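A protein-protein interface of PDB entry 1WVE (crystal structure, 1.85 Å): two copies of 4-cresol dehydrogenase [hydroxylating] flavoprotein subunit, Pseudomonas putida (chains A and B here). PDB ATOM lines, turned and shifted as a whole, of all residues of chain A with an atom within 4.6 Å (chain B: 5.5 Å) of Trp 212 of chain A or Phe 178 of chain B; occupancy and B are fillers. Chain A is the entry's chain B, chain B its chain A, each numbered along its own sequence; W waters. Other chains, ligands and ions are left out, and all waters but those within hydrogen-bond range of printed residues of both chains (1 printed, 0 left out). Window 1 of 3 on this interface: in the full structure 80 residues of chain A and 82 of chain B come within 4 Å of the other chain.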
ATOM      1  N   GLY A 197       7.760  -7.468   4.544  1.00  0.00           N
ATOM      2  CA  GLY A 197       8.151  -8.860   4.710  1.00  0.00           C
ATOM      3  C   GLY A 197       7.300  -9.694   5.649  1.00  0.00           C
ATOM      4  O   GLY A 197       6.083  -9.718   5.540  1.00  0.00           O
ATOM      5  N   PHE A 210      13.804 -13.421   6.446  1.00  0.00           N
ATOM      6  CA  PHE A 210      13.411 -13.557   5.042  1.00  0.00           C
ATOM      7  C   PHE A 210      12.868 -12.215   4.515  1.00  0.00           C
ATOM      8  O   PHE A 210      11.869 -11.678   5.002  1.00  0.00           O
ATOM      9  CB  PHE A 210      12.352 -14.671   4.921  1.00  0.00           C
ATOM     10  CG  PHE A 210      11.852 -14.892   3.518  1.00  0.00           C
ATOM     11  CD1 PHE A 210      12.716 -15.348   2.519  1.00  0.00           C
ATOM     12  CD2 PHE A 210      10.517 -14.663   3.197  1.00  0.00           C
ATOM     13  CE1 PHE A 210      12.251 -15.578   1.217  1.00  0.00           C
ATOM     14  CE2 PHE A 210      10.039 -14.890   1.887  1.00  0.00           C
ATOM     15  CZ  PHE A 210      10.907 -15.348   0.908  1.00  0.00           C
ATOM     16  N   LYS A 211      13.519 -11.691   3.490  1.00  0.00           N
ATOM     17  CA  LYS A 211      13.165 -10.390   2.944  1.00  0.00           C
ATOM     18  C   LYS A 211      11.783 -10.125   2.390  1.00  0.00           C
ATOM     19  O   LYS A 211      11.106  -9.189   2.803  1.00  0.00           O
ATOM     20  CB  LYS A 211      14.138 -10.019   1.826  1.00  0.00           C
ATOM     21  CG  LYS A 211      15.500  -9.560   2.255  1.00  0.00           C
ATOM     22  CD  LYS A 211      16.434  -9.724   1.068  1.00  0.00           C
ATOM     23  CE  LYS A 211      17.159  -8.458   0.699  1.00  0.00           C
ATOM     24  NZ  LYS A 211      16.270  -7.281   0.604  1.00  0.00           N
ATOM     25  N   TRP A 212      11.396 -10.955   1.429  1.00  0.00           N
ATOM     26  CA  TRP A 212      10.187 -10.748   0.657  1.00  0.00           C
ATOM     27  C   TRP A 212       8.820 -10.841   1.282  1.00  0.00           C
ATOM     28  O   TRP A 212       7.936 -10.036   0.948  1.00  0.00           O
ATOM     29  CB  TRP A 212      10.196 -11.671  -0.580  1.00  0.00           C
ATOM     30  CG  TRP A 212      11.532 -11.933  -1.212  1.00  0.00           C
ATOM     31  CD1 TRP A 212      11.999 -13.148  -1.613  1.00  0.00           C
ATOM     32  CD2 TRP A 212      12.561 -10.988  -1.535  1.00  0.00           C
ATOM     33  NE1 TRP A 212      13.237 -13.029  -2.160  1.00  0.00           N
ATOM     34  CE2 TRP A 212      13.618 -11.715  -2.126  1.00  0.00           C
ATOM     35  CE3 TRP A 212      12.693  -9.597  -1.392  1.00  0.00           C
ATOM     36  CZ2 TRP A 212      14.796 -11.108  -2.570  1.00  0.00           C
ATOM     37  CZ3 TRP A 212      13.864  -8.989  -1.837  1.00  0.00           C
ATOM     38  CH2 TRP A 212      14.902  -9.745  -2.418  1.00  0.00           C
ATOM     39  N   GLY A 213       8.622 -11.814   2.168  1.00  0.00           N
ATOM     40  CA  GLY A 213       7.295 -11.984   2.726  1.00  0.00           C
ATOM     41  C   GLY A 213       6.426 -12.563   1.607  1.00  0.00           C
ATOM     42  O   GLY A 213       6.907 -13.340   0.781  1.00  0.00           O
ATOM     43  N   TYR A 214       5.161 -12.163   1.571  1.00  0.00           N
ATOM     44  CA  TYR A 214       4.188 -12.657   0.598  1.00  0.00           C
ATOM     45  C   TYR A 214       3.503 -11.482  -0.097  1.00  0.00           C
ATOM     46  O   TYR A 214       3.278 -10.453   0.525  1.00  0.00           O
ATOM     47  CB  TYR A 214       3.157 -13.511   1.340  1.00  0.00           C
ATOM     48  CG  TYR A 214       1.926 -13.869   0.541  1.00  0.00           C
ATOM     49  CD1 TYR A 214       0.728 -13.174   0.709  1.00  0.00           C
ATOM     50  CD2 TYR A 214       1.951 -14.928  -0.358  1.00  0.00           C
ATOM     51  CE1 TYR A 214      -0.429 -13.542  -0.007  1.00  0.00           C
ATOM     52  CE2 TYR A 214       0.818 -15.300  -1.071  1.00  0.00           C
ATOM     53  CZ  TYR A 214      -0.369 -14.610  -0.893  1.00  0.00           C
ATOM     54  OH  TYR A 214      -1.494 -15.014  -1.589  1.00  0.00           O
ATOM     55  N   THR A 217       6.418  -6.992  -2.492  1.00  0.00           N
ATOM     56  CA  THR A 217       7.418  -6.737  -1.458  1.00  0.00           C
ATOM     57  C   THR A 217       7.776  -5.262  -1.665  1.00  0.00           C
ATOM     58  O   THR A 217       8.292  -4.862  -2.707  1.00  0.00           O
ATOM     59  CB  THR A 217       8.630  -7.719  -1.568  1.00  0.00           C
ATOM     60  OG1 THR A 217       9.601  -7.394  -0.560  1.00  0.00           O
ATOM     61  CG2 THR A 217       9.253  -7.683  -2.954  1.00  0.00           C
ATOM     62  N   THR B 164      10.355 -15.888 -11.541  1.00  0.00           N
ATOM     63  CA  THR B 164      10.768 -14.751 -10.725  1.00  0.00           C
ATOM     64  C   THR B 164       9.584 -13.884 -10.321  1.00  0.00           C
ATOM     65  O   THR B 164       9.606 -13.303  -9.246  1.00  0.00           O
ATOM     66  CB  THR B 164      11.851 -13.911 -11.450  1.00  0.00           C
ATOM     67  OG1 THR B 164      12.949 -14.763 -11.794  1.00  0.00           O
ATOM     68  CG2 THR B 164      12.388 -12.790 -10.539  1.00  0.00           C
ATOM     69  N   ARG B 167       8.625 -15.081  -7.302  1.00  0.00           N
ATOM     70  CA  ARG B 167       9.785 -15.134  -6.408  1.00  0.00           C
ATOM     71  C   ARG B 167      10.232 -16.559  -6.073  1.00  0.00           C
ATOM     72  O   ARG B 167      10.473 -16.900  -4.908  1.00  0.00           O
ATOM     73  CB  ARG B 167       9.523 -14.320  -5.127  1.00  0.00           C
ATOM     74  CG  ARG B 167       9.377 -12.804  -5.412  1.00  0.00           C
ATOM     75  CD  ARG B 167       9.524 -11.949  -4.149  1.00  0.00           C
ATOM     76  NE  ARG B 167       8.488 -12.209  -3.141  1.00  0.00           N
ATOM     77  CZ  ARG B 167       7.371 -11.494  -3.008  1.00  0.00           C
ATOM     78  NH1 ARG B 167       7.126 -10.466  -3.826  1.00  0.00           N
ATOM     79  NH2 ARG B 167       6.511 -11.785  -2.037  1.00  0.00           N
ATOM     80  N   GLY B 168      10.340 -17.371  -7.124  1.00  0.00           N
ATOM     81  CA  GLY B 168      10.777 -18.752  -7.010  1.00  0.00           C
ATOM     82  C   GLY B 168      12.267 -18.855  -6.709  1.00  0.00           C
ATOM     83  O   GLY B 168      12.980 -17.846  -6.697  1.00  0.00           O
ATOM     84  N   GLU B 176      18.534 -17.448  -5.259  1.00  0.00           N
ATOM     85  CA  GLU B 176      17.502 -16.519  -4.822  1.00  0.00           C
ATOM     86  C   GLU B 176      17.244 -15.667  -6.065  1.00  0.00           C
ATOM     87  O   GLU B 176      17.795 -14.580  -6.223  1.00  0.00           O
ATOM     88  CB  GLU B 176      18.015 -15.652  -3.666  1.00  0.00           C
ATOM     89  CG  GLU B 176      16.949 -15.327  -2.623  1.00  0.00           C
ATOM     90  CD  GLU B 176      15.642 -14.893  -3.249  1.00  0.00           C
ATOM     91  OE1 GLU B 176      15.682 -14.006  -4.127  1.00  0.00           O
ATOM     92  OE2 GLU B 176      14.581 -15.435  -2.865  1.00  0.00           O
ATOM     93  N   HIS B 177      16.418 -16.191  -6.964  1.00  0.00           N
ATOM     94  CA  HIS B 177      16.138 -15.505  -8.216  1.00  0.00           C
ATOM     95  C   HIS B 177      15.752 -14.041  -8.175  1.00  0.00           C
ATOM     96  O   HIS B 177      16.318 -13.244  -8.925  1.00  0.00           O
ATOM     97  CB  HIS B 177      15.121 -16.328  -9.006  1.00  0.00           C
ATOM     98  CG  HIS B 177      15.581 -17.731  -9.262  1.00  0.00           C
ATOM     99  ND1 HIS B 177      14.720 -18.755  -9.601  1.00  0.00           N
ATOM    100  CD2 HIS B 177      16.821 -18.285  -9.206  1.00  0.00           C
ATOM    101  CE1 HIS B 177      15.408 -19.878  -9.740  1.00  0.00           C
ATOM    102  NE2 HIS B 177      16.684 -19.620  -9.503  1.00  0.00           N
ATOM    103  N   PHE B 178      14.823 -13.652  -7.307  1.00  0.00           N
ATOM    104  CA  PHE B 178      14.457 -12.242  -7.299  1.00  0.00           C
ATOM    105  C   PHE B 178      15.662 -11.382  -6.914  1.00  0.00           C
ATOM    106  O   PHE B 178      15.830 -10.283  -7.426  1.00  0.00           O
ATOM    107  CB  PHE B 178      13.286 -11.947  -6.341  1.00  0.00           C
ATOM    108  CG  PHE B 178      12.840 -10.503  -6.372  1.00  0.00           C
ATOM    109  CD1 PHE B 178      12.635  -9.792  -5.187  1.00  0.00           C
ATOM    110  CD2 PHE B 178      12.686  -9.831  -7.590  1.00  0.00           C
ATOM    111  CE1 PHE B 178      12.293  -8.428  -5.208  1.00  0.00           C
ATOM    112  CE2 PHE B 178      12.340  -8.464  -7.628  1.00  0.00           C
ATOM    113  CZ  PHE B 178      12.148  -7.760  -6.429  1.00  0.00           C
ATOM    114  N   MET B 179      16.497 -11.903  -6.021  1.00  0.00           N
ATOM    115  CA  MET B 179      17.684 -11.189  -5.561  1.00  0.00           C
ATOM    116  C   MET B 179      18.643 -10.906  -6.721  1.00  0.00           C
ATOM    117  O   MET B 179      19.295  -9.867  -6.759  1.00  0.00           O
ATOM    118  CB  MET B 179      18.389 -12.014  -4.470  1.00  0.00           C
ATOM    119  CG  MET B 179      19.648 -11.388  -3.884  1.00  0.00           C
ATOM    120  SD  MET B 179      20.433 -12.458  -2.622  1.00  0.00           S
ATOM    121  CE  MET B 179      21.422 -13.520  -3.678  1.00  0.00           C
ATOM    122  N   MET B 180      18.713 -11.828  -7.674  1.00  0.00           N
ATOM    123  CA  MET B 180      19.596 -11.677  -8.824  1.00  0.00           C
ATOM    124  C   MET B 180      18.922 -11.014 -10.050  1.00  0.00           C
ATOM    125  O   MET B 180      19.550 -10.811 -11.098  1.00  0.00           O
ATOM    126  CB  MET B 180      20.167 -13.053  -9.191  1.00  0.00           C
ATOM    127  CG  MET B 180      20.990 -13.689  -8.061  1.00  0.00           C
ATOM    128  SD  MET B 180      22.434 -12.669  -7.595  1.00  0.00           S
ATOM    129  CE  MET B 180      21.801 -11.629  -6.386  1.00  0.00           C
ATOM    130  N   GLN B 181      17.644 -10.676  -9.921  1.00  0.00           N
ATOM    131  CA  GLN B 181      16.906 -10.026 -11.003  1.00  0.00           C
ATOM    132  C   GLN B 181      17.366  -8.560 -11.083  1.00  0.00           C
ATOM    133  O   GLN B 181      17.640  -7.938 -10.062  1.00  0.00           O
ATOM    134  CB  GLN B 181      15.396 -10.112 -10.719  1.00  0.00           C
ATOM    135  CG  GLN B 181      14.484  -9.384 -11.715  1.00  0.00           C
ATOM    136  CD  GLN B 181      14.207  -7.933 -11.311  1.00  0.00           C
ATOM    137  OE1 GLN B 181      14.136  -7.612 -10.125  1.00  0.00           O
ATOM    138  NE2 GLN B 181      14.030  -7.067 -12.292  1.00  0.00           N
ATOM    139  N   MET B 184      13.335  -4.489 -15.123  1.00  0.00           N
ATOM    140  CA  MET B 184      12.078  -5.123 -15.462  1.00  0.00           C
ATOM    141  C   MET B 184      11.235  -4.137 -16.261  1.00  0.00           C
ATOM    142  O   MET B 184      11.289  -2.935 -16.030  1.00  0.00           O
ATOM    143  CB  MET B 184      11.334  -5.509 -14.174  1.00  0.00           C
ATOM    144  CG  MET B 184       9.963  -6.144 -14.354  1.00  0.00           C
ATOM    145  SD  MET B 184       9.073  -6.347 -12.735  1.00  0.00           S
ATOM    146  CE  MET B 184      10.270  -7.294 -11.838  1.00  0.00           C
ATOM    147  N   LYS B 211      20.627  -2.382 -10.136  1.00  0.00           N
ATOM    148  CA  LYS B 211      19.230  -2.627  -9.775  1.00  0.00           C
ATOM    149  C   LYS B 211      18.282  -1.493  -9.448  1.00  0.00           C
ATOM    150  O   LYS B 211      17.203  -1.381 -10.035  1.00  0.00           O
ATOM    151  CB  LYS B 211      19.152  -3.582  -8.575  1.00  0.00           C
ATOM    152  CG  LYS B 211      19.467  -5.020  -8.879  1.00  0.00           C
ATOM    153  CD  LYS B 211      19.787  -5.814  -7.586  1.00  0.00           C
ATOM    154  CE  LYS B 211      18.573  -6.115  -6.738  1.00  0.00           C
ATOM    155  NZ  LYS B 211      17.632  -7.090  -7.338  1.00  0.00           N
ATOM    156  N   ASP B 219      10.653  -2.917  -8.616  1.00  0.00           N
ATOM    157  CA  ASP B 219      10.588  -4.315  -9.066  1.00  0.00           C
ATOM    158  C   ASP B 219       9.831  -5.212  -8.071  1.00  0.00           C
ATOM    159  O   ASP B 219       8.959  -6.004  -8.457  1.00  0.00           O
ATOM    160  CB  ASP B 219      12.004  -4.868  -9.283  1.00  0.00           C
ATOM    161  CG  ASP B 219      12.844  -3.980 -10.180  1.00  0.00           C
ATOM    162  OD1 ASP B 219      13.196  -2.864  -9.742  1.00  0.00           O
ATOM    163  OD2 ASP B 219      13.150  -4.389 -11.319  1.00  0.00           O
ATOM    164  N   GLY B 220      10.165  -5.082  -6.791  1.00  0.00           N
ATOM    165  CA  GLY B 220       9.515  -5.887  -5.768  1.00  0.00           C
ATOM    166  C   GLY B 220       8.008  -5.696  -5.726  1.00  0.00           C
ATOM    167  O   GLY B 220       7.253  -6.645  -5.511  1.00  0.00           O
ATOM    168  N   THR B 223       6.336  -8.079  -8.225  1.00  0.00           N
ATOM    169  CA  THR B 223       6.409  -9.511  -7.968  1.00  0.00           C
ATOM    170  C   THR B 223       5.283  -9.918  -7.018  1.00  0.00           C
ATOM    171  O   THR B 223       4.945  -9.175  -6.093  1.00  0.00           O
ATOM    172  CB  THR B 223       7.801  -9.924  -7.393  1.00  0.00           C
ATOM    173  OG1 THR B 223       8.036  -9.257  -6.152  1.00  0.00           O
ATOM    174  CG2 THR B 223       8.921  -9.535  -8.383  1.00  0.00           C
HETATM  175  O   HOH W   1       8.110 -14.487  -1.374  1.00  0.00           O
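O of Gly 220 of chain B lies within hydrogen-bond range of N of Thr 217 of chain A (3.2 Å).
OE2 of Glu 176 of chain B lies within hydrogen-bond range of NE1 of Trp 212 of chain A, 2.8 Å away.
The backbone carbonyl oxygen (O) of Gly 213 of chain A lies within hydrogen-bond range of the guanidinium group (NH2) of Arg 167 of chain B, at 3.2 Å.
Water W1 bridges the backbone carbonyl oxygen of Gly 213 of chain A (2.7 Å) and the guanidinium group of Arg 167 of chain B (2.9 Å).
OG1 of Thr 217 of chain A lies within hydrogen-bond range of O of Trp 212 of chain A, at 3.5 Å.
The side-chain hydroxyl of Thr 223 of chain B is in hydrogen-bond range of the backbone carbonyl oxygen of Gly 220 of chain B (2.8 Å).
The side-chain hydroxyl of Thr 223 of chain B lies within hydrogen-bond range of the guanidinium group of Arg 167 of chain B, at 2.8 Å.
The backbone NH (N) of Phe 178 of chain B lies within hydrogen-bond range of the side-chain carboxylate (OE1) of Glu 176 of chain B (3.3 Å).
O of Met 179 of chain B is in hydrogen-bond range of NZ of Lys 211 of chain B (3.3 Å).
The side-chain carboxylate (OE1) of Glu 176 of chain B is in hydrogen-bond range of the backbone NH (N) of Met 179 of chain B (2.9 Å).
Among the printed residues, merely in contact across the chains: Trp 212 of chain A with Arg 167 of chain B (3.1 Å), Trp 212 of chain A with Phe 178 of chain B (3.6 Å), Trp 212 of chain A with Met 179 of chain B (3.9 Å), Tyr 214 of chain A with Arg 167 of chain B (3.6 Å), Thr 217 of chain A with Arg 167 of chain B (3.6 Å), Thr 217 of chain A with Phe 178 of chain B (3.9 Å) and Thr 217 of chain A with Thr 223 of chain B (3.8 Å).
Hydrophobic or aromatic side chains of chain B within 4 Å of the printed part of chain A: Phe 178.
Printed residues of chain A that touch a printed residue of chain B: Trp 212, Gly 213, Tyr 214 and Thr 217.
Hydrophobic or aromatic side chains of chain A that line the printed part of chain B: Trp 212.
Along chain A the printed residues that touch a printed residue of chain B span positions 212 to 217.
Among the printed residues, 10 pairs touch across the chains.
1 position is printed for both chains.
Printed residues of chain B within 4 Å of Trp 212 of chain A: Arg 167 (3.1 Å), Glu 176 (2.8 Å), Phe 178 (3.6 Å) and Met 179 (3.9 Å).
Of the printed residues of chain B, Thr 217 of chain A touches Arg 167, Phe 178, Gly 220 and Thr 223.
Printed residues of chain A within 4 Å of Arg 167 of chain B: Trp 212, Gly 213, Tyr 214 and Thr 217.
Phe 178 of chain B touches just these residues of chain A: Trp 212 and Thr 217.
Of the printed residues of chain A, Gly 220 of chain B touches Thr 217 (3.1 Å).
Printed residues of chain A within 4 Å of Thr 223 of chain B: Thr 217.
The nearest printed residue of chain B that does not touch Trp 212 of chain A is Lys 211 of chain B (6.2 Å).
The nearest printed residue of chain A that does not touch Arg 167 of chain B is Phe 210 of chain A (5.7 Å).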
